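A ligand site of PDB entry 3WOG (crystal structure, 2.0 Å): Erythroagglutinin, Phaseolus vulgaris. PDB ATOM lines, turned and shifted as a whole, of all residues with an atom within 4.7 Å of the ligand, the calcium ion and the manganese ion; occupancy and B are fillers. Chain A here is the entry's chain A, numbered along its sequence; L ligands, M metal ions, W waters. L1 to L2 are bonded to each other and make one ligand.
The side-chain carboxylate (OE2) of Glu 124 lies close to the side-chain hydroxyl (OG) of Ser 149 (3.5 Å). The side-chain carboxylate of Asp 134 sits close to the indole nitrogen of Trp 133, at 3.4 Å. N of Gly 104 sits at hydrogen-bond distance from OD2 of Asp 86 (3.5 Å). The backbone carbonyl oxygen (O) of Thr 216 lies within hydrogen-bond range of the side-chain amide nitrogen (ND2) of Asn 219 (3.1 Å). The backbone carbonyl oxygen (O) of Asn 219 lies close to the backbone NH (N) of Gly 214, 3.2 Å away.
OD1 of Asn 130 binds the calcium ion, at 2.3 Å. The side-chain carboxylate (OD2) of Asp 134 binds the calcium ion, at 2.3 Å. The calcium ion is bound by water W5 (2.3 Å). The calcium ion is bound by OD1 of Asp 126, at 2.3 Å. Water W4 is bound to the calcium ion (2.3 Å). O of Leu 128 binds the calcium ion, 2.4 Å away. The side-chain carboxylate (OD2) of Asp 126 is bound to the calcium ion. The calcium ion has seven donor atoms within binding distance.
CA of Gly 103 touches O3 of LIG L1, 3.5 Å away. N of Leu 105 touches O4 of LIG L1, 3.8 Å away. N of Val 131 touches O5 of LG2 L2, 3.8 Å away. His 132 touches the ligand. Trp 133 touches the ligand. Gly 214 touches the ligand. ND2 of Asn 219 touches C6 of LG2 L2 (3.7 Å). Hydrophobic or aromatic side chains that line the ligand: Leu 105, Leu 128, Val 131, His 132, Trp 133 and Ile 215. Along chain A the residues within 4 Å of the ligand span positions 103 to 219. The nearest printed residue that does not touch the ligand is Lys 102 (4.2 Å).
Four residues have an atom within 4 Å of the calcium ion: Asp 126, Leu 128, Asn 130 and Asp 134.
Of the 22 residues printed, 4 come within 4 Å of the manganese ion.
The manganese ion is bound by water W1, water W2, a ring nitrogen (NE2) of His 139, the side-chain carboxylate of Asp 126, the side-chain carboxylate of Glu 124 and the side-chain carboxylate of Asp 134. The manganese ion has six donor atoms within binding distance.
The side-chain amide nitrogen (ND2) of Asn 130 sits at hydrogen-bond distance from an oxygen (O5) of LG2 L2 (3.1 Å). An oxygen (O3) of LIG L1 is in hydrogen-bond range of the backbone NH of Gly 104, 2.9 Å away. N of Thr 216 lies within hydrogen-bond range of O4 of LG2 L2. An oxygen (O4) of LG2 L2 is in hydrogen-bond range of the backbone NH (N) of Ile 215, 3.3 Å away.
Water W4 lies within hydrogen-bond range of O of Gly 104 (2.9 Å) and NE1 of Trp 133 (3.0 Å). Water W1 lies within hydrogen-bond range of OE1 of Glu 124 (2.7 Å), O of Ile 147 (3.0 Å) and NE1 of Trp 133 (3.4 Å). Water W6 lies within hydrogen-bond range of the side-chain carboxylate of Asp 86 (2.6 Å), an oxygen (O3) of LIG L1 (2.6 Å), the side-chain amide nitrogen of Asn 130 (2.8 Å) and the backbone NH of Gly 104 (3.3 Å). Water W3 lies within hydrogen-bond range of O1 of LG2 L2 (2.7 Å), O of Tyr 129 (2.8 Å) and N of Val 131 (2.9 Å). Water W7 lies within hydrogen-bond range of an oxygen (O5) of LG2 L2 (2.8 Å), the backbone NH of His 132 (2.9 Å) and the backbone NH of Val 131 (3.4 Å).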
ATOM      1  N   ASP A  86     -19.634  21.979  29.359  1.00  0.00           N
ATOM      2  CA  ASP A  86     -18.797  23.182  29.170  1.00  0.00           C
ATOM      3  C   ASP A  86     -17.908  23.510  30.373  1.00  0.00           C
ATOM      4  O   ASP A  86     -16.891  24.186  30.255  1.00  0.00           O
ATOM      5  CB  ASP A  86     -19.686  24.374  28.885  1.00  0.00           C
ATOM      6  CG  ASP A  86     -19.896  24.580  27.419  1.00  0.00           C
ATOM      7  OD1 ASP A  86     -18.930  25.011  26.740  1.00  0.00           O
ATOM      8  OD2 ASP A  86     -21.028  24.290  26.951  1.00  0.00           O
ATOM      9  N   LYS A 102     -26.807  29.552  28.728  1.00  0.00           N
ATOM     10  CA  LYS A 102     -26.219  28.236  28.931  1.00  0.00           C
ATOM     11  C   LYS A 102     -24.900  28.040  28.130  1.00  0.00           C
ATOM     12  O   LYS A 102     -24.284  29.021  27.688  1.00  0.00           O
ATOM     13  CB  LYS A 102     -27.252  27.162  28.593  1.00  0.00           C
ATOM     14  CG  LYS A 102     -27.802  27.279  27.176  1.00  0.00           C
ATOM     15  CD  LYS A 102     -28.673  26.078  26.822  1.00  0.00           C
ATOM     16  CE  LYS A 102     -30.048  26.152  27.476  1.00  0.00           C
ATOM     17  NZ  LYS A 102     -30.818  24.878  27.334  1.00  0.00           N
ATOM     18  N   GLY A 103     -24.452  26.795  27.978  1.00  0.00           N
ATOM     19  CA  GLY A 103     -23.233  26.510  27.214  1.00  0.00           C
ATOM     20  C   GLY A 103     -22.000  27.193  27.760  1.00  0.00           C
ATOM     21  O   GLY A 103     -21.772  27.213  28.972  1.00  0.00           O
ATOM     22  N   GLY A 104     -21.188  27.768  26.874  1.00  0.00           N
ATOM     23  CA  GLY A 104     -19.923  28.374  27.280  1.00  0.00           C
ATOM     24  C   GLY A 104     -20.033  29.608  28.163  1.00  0.00           C
ATOM     25  O   GLY A 104     -19.039  30.079  28.692  1.00  0.00           O
ATOM     26  N   LEU A 105     -21.225  30.166  28.308  1.00  0.00           N
ATOM     27  CA  LEU A 105     -21.430  31.300  29.213  1.00  0.00           C
ATOM     28  C   LEU A 105     -21.697  30.861  30.664  1.00  0.00           C
ATOM     29  O   LEU A 105     -21.850  31.695  31.574  1.00  0.00           O
ATOM     30  CB  LEU A 105     -22.549  32.199  28.660  1.00  0.00           C
ATOM     31  CG  LEU A 105     -22.202  32.794  27.284  1.00  0.00           C
ATOM     32  CD1 LEU A 105     -23.372  33.576  26.662  1.00  0.00           C
ATOM     33  CD2 LEU A 105     -20.968  33.665  27.349  1.00  0.00           C
ATOM     34  N   TYR A 112     -20.243  37.682  25.645  1.00  0.00           N
ATOM     35  CA  TYR A 112     -18.867  37.652  26.094  1.00  0.00           C
ATOM     36  C   TYR A 112     -18.176  38.987  26.307  1.00  0.00           C
ATOM     37  O   TYR A 112     -16.954  39.046  26.434  1.00  0.00           O
ATOM     38  CB  TYR A 112     -17.991  36.713  25.260  1.00  0.00           C
ATOM     39  CG  TYR A 112     -18.015  36.895  23.757  1.00  0.00           C
ATOM     40  CD1 TYR A 112     -16.999  37.607  23.095  1.00  0.00           C
ATOM     41  CD2 TYR A 112     -19.019  36.304  22.977  1.00  0.00           C
ATOM     42  CE1 TYR A 112     -17.004  37.746  21.712  1.00  0.00           C
ATOM     43  CE2 TYR A 112     -19.030  36.423  21.595  1.00  0.00           C
ATOM     44  CZ  TYR A 112     -18.034  37.143  20.973  1.00  0.00           C
ATOM     45  OH  TYR A 112     -18.062  37.248  19.596  1.00  0.00           O
ATOM     46  N   GLU A 124     -13.712  29.485  37.433  1.00  0.00           N
ATOM     47  CA  GLU A 124     -14.221  28.525  36.466  1.00  0.00           C
ATOM     48  C   GLU A 124     -13.265  27.369  36.229  1.00  0.00           C
ATOM     49  O   GLU A 124     -12.038  27.523  36.282  1.00  0.00           O
ATOM     50  CB  GLU A 124     -14.508  29.215  35.104  1.00  0.00           C
ATOM     51  CG  GLU A 124     -13.312  29.828  34.384  1.00  0.00           C
ATOM     52  CD  GLU A 124     -13.639  30.234  32.944  1.00  0.00           C
ATOM     53  OE1 GLU A 124     -14.712  30.869  32.749  1.00  0.00           O
ATOM     54  OE2 GLU A 124     -12.873  29.873  31.995  1.00  0.00           O
ATOM     55  N   ASP A 126     -13.008  25.193  33.158  1.00  0.00           N
ATOM     56  CA  ASP A 126     -13.568  25.336  31.795  1.00  0.00           C
ATOM     57  C   ASP A 126     -13.018  24.187  30.953  1.00  0.00           C
ATOM     58  O   ASP A 126     -11.806  24.068  30.756  1.00  0.00           O
ATOM     59  CB  ASP A 126     -13.139  26.734  31.222  1.00  0.00           C
ATOM     60  CG  ASP A 126     -13.818  27.083  29.894  1.00  0.00           C
ATOM     61  OD1 ASP A 126     -14.336  26.148  29.261  1.00  0.00           O
ATOM     62  OD2 ASP A 126     -13.808  28.312  29.485  1.00  0.00           O
ATOM     63  N   LEU A 128     -14.052  23.388  27.762  1.00  0.00           N
ATOM     64  CA  LEU A 128     -14.245  23.535  26.322  1.00  0.00           C
ATOM     65  C   LEU A 128     -13.785  24.898  25.827  1.00  0.00           C
ATOM     66  O   LEU A 128     -14.247  25.944  26.304  1.00  0.00           O
ATOM     67  CB  LEU A 128     -15.711  23.290  25.957  1.00  0.00           C
ATOM     68  CG  LEU A 128     -15.940  23.394  24.434  1.00  0.00           C
ATOM     69  CD1 LEU A 128     -16.570  22.130  23.881  1.00  0.00           C
ATOM     70  CD2 LEU A 128     -16.657  24.668  23.996  1.00  0.00           C
ATOM     71  N   TYR A 129     -12.855  24.853  24.866  1.00  0.00           N
ATOM     72  CA  TYR A 129     -12.342  26.036  24.188  1.00  0.00           C
ATOM     73  C   TYR A 129     -13.415  26.791  23.396  1.00  0.00           C
ATOM     74  O   TYR A 129     -13.992  26.276  22.435  1.00  0.00           O
ATOM     75  CB  TYR A 129     -11.185  25.625  23.266  1.00  0.00           C
ATOM     76  CG  TYR A 129     -10.702  26.657  22.248  1.00  0.00           C
ATOM     77  CD1 TYR A 129     -10.109  27.847  22.663  1.00  0.00           C
ATOM     78  CD2 TYR A 129     -10.789  26.397  20.878  1.00  0.00           C
ATOM     79  CE1 TYR A 129      -9.629  28.780  21.736  1.00  0.00           C
ATOM     80  CE2 TYR A 129     -10.330  27.307  19.936  1.00  0.00           C
ATOM     81  CZ  TYR A 129      -9.744  28.495  20.364  1.00  0.00           C
ATOM     82  OH  TYR A 129      -9.276  29.386  19.440  1.00  0.00           O
ATOM     83  N   ASN A 130     -13.680  28.022  23.806  1.00  0.00           N
ATOM     84  CA  ASN A 130     -14.616  28.870  23.104  1.00  0.00           C
ATOM     85  C   ASN A 130     -13.801  29.904  22.356  1.00  0.00           C
ATOM     86  O   ASN A 130     -13.166  30.780  22.982  1.00  0.00           O
ATOM     87  CB  ASN A 130     -15.581  29.534  24.088  1.00  0.00           C
ATOM     88  CG  ASN A 130     -16.594  28.566  24.651  1.00  0.00           C
ATOM     89  OD1 ASN A 130     -16.464  28.095  25.798  1.00  0.00           O
ATOM     90  ND2 ASN A 130     -17.607  28.229  23.851  1.00  0.00           N
ATOM     91  N   VAL A 131     -13.783  29.775  21.023  1.00  0.00           N
ATOM     92  CA  VAL A 131     -12.860  30.539  20.168  1.00  0.00           C
ATOM     93  C   VAL A 131     -12.834  32.060  20.406  1.00  0.00           C
ATOM     94  O   VAL A 131     -11.783  32.712  20.280  1.00  0.00           O
ATOM     95  CB  VAL A 131     -13.139  30.239  18.660  1.00  0.00           C
ATOM     96  CG1 VAL A 131     -14.536  30.694  18.249  1.00  0.00           C
ATOM     97  CG2 VAL A 131     -12.084  30.875  17.781  1.00  0.00           C
ATOM     98  N   HIS A 132     -13.979  32.652  20.738  1.00  0.00           N
ATOM     99  CA  HIS A 132     -14.048  34.107  20.864  1.00  0.00           C
ATOM    100  C   HIS A 132     -13.470  34.639  22.155  1.00  0.00           C
ATOM    101  O   HIS A 132     -13.319  35.850  22.299  1.00  0.00           O
ATOM    102  CB  HIS A 132     -15.460  34.618  20.681  1.00  0.00           C
ATOM    103  CG  HIS A 132     -16.029  34.351  19.299  1.00  0.00           C
ATOM    104  ND1 HIS A 132     -15.362  34.648  18.163  1.00  0.00           N
ATOM    105  CD2 HIS A 132     -17.260  33.825  18.907  1.00  0.00           C
ATOM    106  CE1 HIS A 132     -16.115  34.311  17.093  1.00  0.00           C
ATOM    107  NE2 HIS A 132     -17.287  33.801  17.554  1.00  0.00           N
ATOM    108  N   TRP A 133     -13.132  33.771  23.121  1.00  0.00           N
ATOM    109  CA  TRP A 133     -12.550  34.312  24.368  1.00  0.00           C
ATOM    110  C   TRP A 133     -11.618  33.439  25.154  1.00  0.00           C
ATOM    111  O   TRP A 133     -10.853  33.961  25.961  1.00  0.00           O
ATOM    112  CB  TRP A 133     -13.637  34.829  25.295  1.00  0.00           C
ATOM    113  CG  TRP A 133     -14.530  33.725  25.809  1.00  0.00           C
ATOM    114  CD1 TRP A 133     -14.272  32.829  26.848  1.00  0.00           C
ATOM    115  CD2 TRP A 133     -15.845  33.358  25.301  1.00  0.00           C
ATOM    116  NE1 TRP A 133     -15.329  31.958  27.015  1.00  0.00           N
ATOM    117  CE2 TRP A 133     -16.307  32.219  26.120  1.00  0.00           C
ATOM    118  CE3 TRP A 133     -16.685  33.836  24.292  1.00  0.00           C
ATOM    119  CZ2 TRP A 133     -17.535  31.618  25.907  1.00  0.00           C
ATOM    120  CZ3 TRP A 133     -17.929  33.218  24.100  1.00  0.00           C
ATOM    121  CH2 TRP A 133     -18.337  32.150  24.894  1.00  0.00           C
ATOM    122  N   ASP A 134     -11.681  32.113  24.987  1.00  0.00           N
ATOM    123  CA  ASP A 134     -10.886  31.200  25.837  1.00  0.00           C
ATOM    124  C   ASP A 134      -9.450  31.021  25.367  1.00  0.00           C
ATOM    125  O   ASP A 134      -9.180  31.095  24.155  1.00  0.00           O
ATOM    126  CB  ASP A 134     -11.522  29.813  25.870  1.00  0.00           C
ATOM    127  CG  ASP A 134     -12.629  29.679  26.926  1.00  0.00           C
ATOM    128  OD1 ASP A 134     -12.569  30.269  28.064  1.00  0.00           O
ATOM    129  OD2 ASP A 134     -13.567  28.919  26.595  1.00  0.00           O
ATOM    130  N   HIS A 139      -8.602  24.908  31.246  1.00  0.00           N
ATOM    131  CA  HIS A 139      -8.032  25.940  32.110  1.00  0.00           C
ATOM    132  C   HIS A 139      -8.821  26.179  33.373  1.00  0.00           C
ATOM    133  O   HIS A 139     -10.021  25.945  33.406  1.00  0.00           O
ATOM    134  CB  HIS A 139      -7.866  27.265  31.320  1.00  0.00           C
ATOM    135  CG  HIS A 139      -9.153  27.785  30.669  1.00  0.00           C
ATOM    136  ND1 HIS A 139      -9.575  27.374  29.466  1.00  0.00           N
ATOM    137  CD2 HIS A 139     -10.071  28.764  31.100  1.00  0.00           C
ATOM    138  CE1 HIS A 139     -10.716  28.004  29.134  1.00  0.00           C
ATOM    139  NE2 HIS A 139     -11.028  28.868  30.138  1.00  0.00           N
ATOM    140  N   ILE A 147     -17.097  36.450  31.051  1.00  0.00           N
ATOM    141  CA  ILE A 147     -16.702  35.075  30.720  1.00  0.00           C
ATOM    142  C   ILE A 147     -15.238  35.029  30.258  1.00  0.00           C
ATOM    143  O   ILE A 147     -14.597  33.964  30.240  1.00  0.00           O
ATOM    144  CB  ILE A 147     -17.662  34.449  29.665  1.00  0.00           C
ATOM    145  CG1 ILE A 147     -17.640  32.909  29.698  1.00  0.00           C
ATOM    146  CG2 ILE A 147     -17.352  34.967  28.258  1.00  0.00           C
ATOM    147  CD1 ILE A 147     -17.916  32.293  31.062  1.00  0.00           C
ATOM    148  N   SER A 149     -11.835  35.376  31.235  1.00  0.00           N
ATOM    149  CA  SER A 149     -11.129  35.375  32.520  1.00  0.00           C
ATOM    150  C   SER A 149     -10.046  36.441  32.590  1.00  0.00           C
ATOM    151  O   SER A 149      -9.333  36.685  31.604  1.00  0.00           O
ATOM    152  CB  SER A 149     -10.523  34.000  32.816  1.00  0.00           C
ATOM    153  OG  SER A 149     -11.492  32.976  32.618  1.00  0.00           O
ATOM    154  N   GLY A 214     -22.528  20.861  27.051  1.00  0.00           N
ATOM    155  CA  GLY A 214     -22.442  21.401  25.683  1.00  0.00           C
ATOM    156  C   GLY A 214     -23.801  21.460  25.019  1.00  0.00           C
ATOM    157  O   GLY A 214     -24.711  20.695  25.349  1.00  0.00           O
ATOM    158  N   ILE A 215     -23.959  22.391  24.091  1.00  0.00           N
ATOM    159  CA  ILE A 215     -25.179  22.447  23.317  1.00  0.00           C
ATOM    160  C   ILE A 215     -25.109  21.517  22.084  1.00  0.00           C
ATOM    161  O   ILE A 215     -26.146  21.076  21.584  1.00  0.00           O
ATOM    162  CB  ILE A 215     -25.623  23.892  22.967  1.00  0.00           C
ATOM    163  CG1 ILE A 215     -24.684  24.544  21.942  1.00  0.00           C
ATOM    164  CG2 ILE A 215     -25.725  24.754  24.229  1.00  0.00           C
ATOM    165  CD1 ILE A 215     -25.337  25.699  21.197  1.00  0.00           C
ATOM    166  N   THR A 216     -23.906  21.201  21.618  1.00  0.00           N
ATOM    167  CA  THR A 216     -23.698  20.433  20.396  1.00  0.00           C
ATOM    168  C   THR A 216     -23.360  18.982  20.702  1.00  0.00           C
ATOM    169  O   THR A 216     -22.445  18.706  21.469  1.00  0.00           O
ATOM    170  CB  THR A 216     -22.583  21.051  19.524  1.00  0.00           C
ATOM    171  OG1 THR A 216     -22.941  22.404  19.210  1.00  0.00           O
ATOM    172  CG2 THR A 216     -22.405  20.299  18.214  1.00  0.00           C
ATOM    173  N   ASN A 219     -20.336  16.922  22.824  1.00  0.00           N
ATOM    174  CA  ASN A 219     -19.686  17.786  23.808  1.00  0.00           C
ATOM    175  C   ASN A 219     -20.541  17.821  25.080  1.00  0.00           C
ATOM    176  O   ASN A 219     -21.545  18.513  25.128  1.00  0.00           O
ATOM    177  CB  ASN A 219     -19.508  19.196  23.233  1.00  0.00           C
ATOM    178  CG  ASN A 219     -18.723  19.198  21.935  1.00  0.00           C
ATOM    179  OD1 ASN A 219     -17.496  19.208  21.944  1.00  0.00           O
ATOM    180  ND2 ASN A 219     -19.433  19.208  20.814  1.00  0.00           N
HETATM  181  C1  LIG L   1     -22.071  28.698  20.607  1.00  0.00           C
HETATM  182  C2  LIG L   1     -21.776  27.681  21.717  1.00  0.00           C
HETATM  183  C3  LIG L   1     -22.166  28.247  23.078  1.00  0.00           C
HETATM  184  C4  LIG L   1     -21.393  29.552  23.317  1.00  0.00           C
HETATM  185  C5  LIG L   1     -21.679  30.511  22.164  1.00  0.00           C
HETATM  186  C6  LIG L   1     -20.840  31.786  22.223  1.00  0.00           C
HETATM  187  O1  LIG L   1     -23.461  28.944  20.458  1.00  0.00           O
HETATM  188  O2  LIG L   1     -20.386  27.437  21.759  1.00  0.00           O
HETATM  189  O3  LIG L   1     -21.844  27.293  24.080  1.00  0.00           O
HETATM  190  O4  LIG L   1     -21.701  30.123  24.570  1.00  0.00           O
HETATM  191  O5  LIG L   1     -21.396  29.909  20.900  1.00  0.00           O
HETATM  192  O6  LIG L   1     -21.571  32.803  21.562  1.00  0.00           O
HETATM  193  C1  LG2 L   2     -20.010  26.300  20.967  1.00  0.00           C
HETATM  194  C2  LG2 L   2     -18.631  26.576  20.378  1.00  0.00           C
HETATM  195  C3  LG2 L   2     -18.064  25.371  19.586  1.00  0.00           C
HETATM  196  C4  LG2 L   2     -18.240  24.068  20.382  1.00  0.00           C
HETATM  197  C5  LG2 L   2     -19.674  23.936  20.943  1.00  0.00           C
HETATM  198  C6  LG2 L   2     -19.840  22.718  21.845  1.00  0.00           C
HETATM  199  C7  LG2 L   2     -18.199  28.919  19.885  1.00  0.00           C
HETATM  200  C8  LG2 L   2     -18.411  30.013  18.874  1.00  0.00           C
HETATM  201  N1  LG2 L   2     -18.735  27.743  19.545  1.00  0.00           N
HETATM  202  O1  LG2 L   2     -16.693  25.560  19.276  1.00  0.00           O
HETATM  203  O2  LG2 L   2     -17.856  22.964  19.566  1.00  0.00           O
HETATM  204  O3  LG2 L   2     -20.035  25.093  21.697  1.00  0.00           O
HETATM  205  O4  LG2 L   2     -21.192  22.592  22.257  1.00  0.00           O
HETATM  206  O5  LG2 L   2     -17.547  29.115  20.928  1.00  0.00           O
HETATM  207 CA    CA M   1     -15.172  27.632  27.663  1.00  0.00          CA
HETATM  208 MN    MN M   2     -12.718  29.884  30.014  1.00  0.00          MN
HETATM  209  O   HOH W   1     -14.284  31.026  30.083  1.00  0.00           O
HETATM  210  O   HOH W   2     -11.686  31.499  30.344  1.00  0.00           O
HETATM  211  O   HOH W   3     -14.745  27.253  19.906  1.00  0.00           O
HETATM  212  O   HOH W   4     -16.225  29.508  28.589  1.00  0.00           O
HETATM  213  O   HOH W   5     -16.963  26.216  28.108  1.00  0.00           O
HETATM  214  O   HOH W   6     -19.485  26.192  24.499  1.00  0.00           O
HETATM  215  O   HOH W   7     -16.578  31.652  21.453  1.00  0.00           O
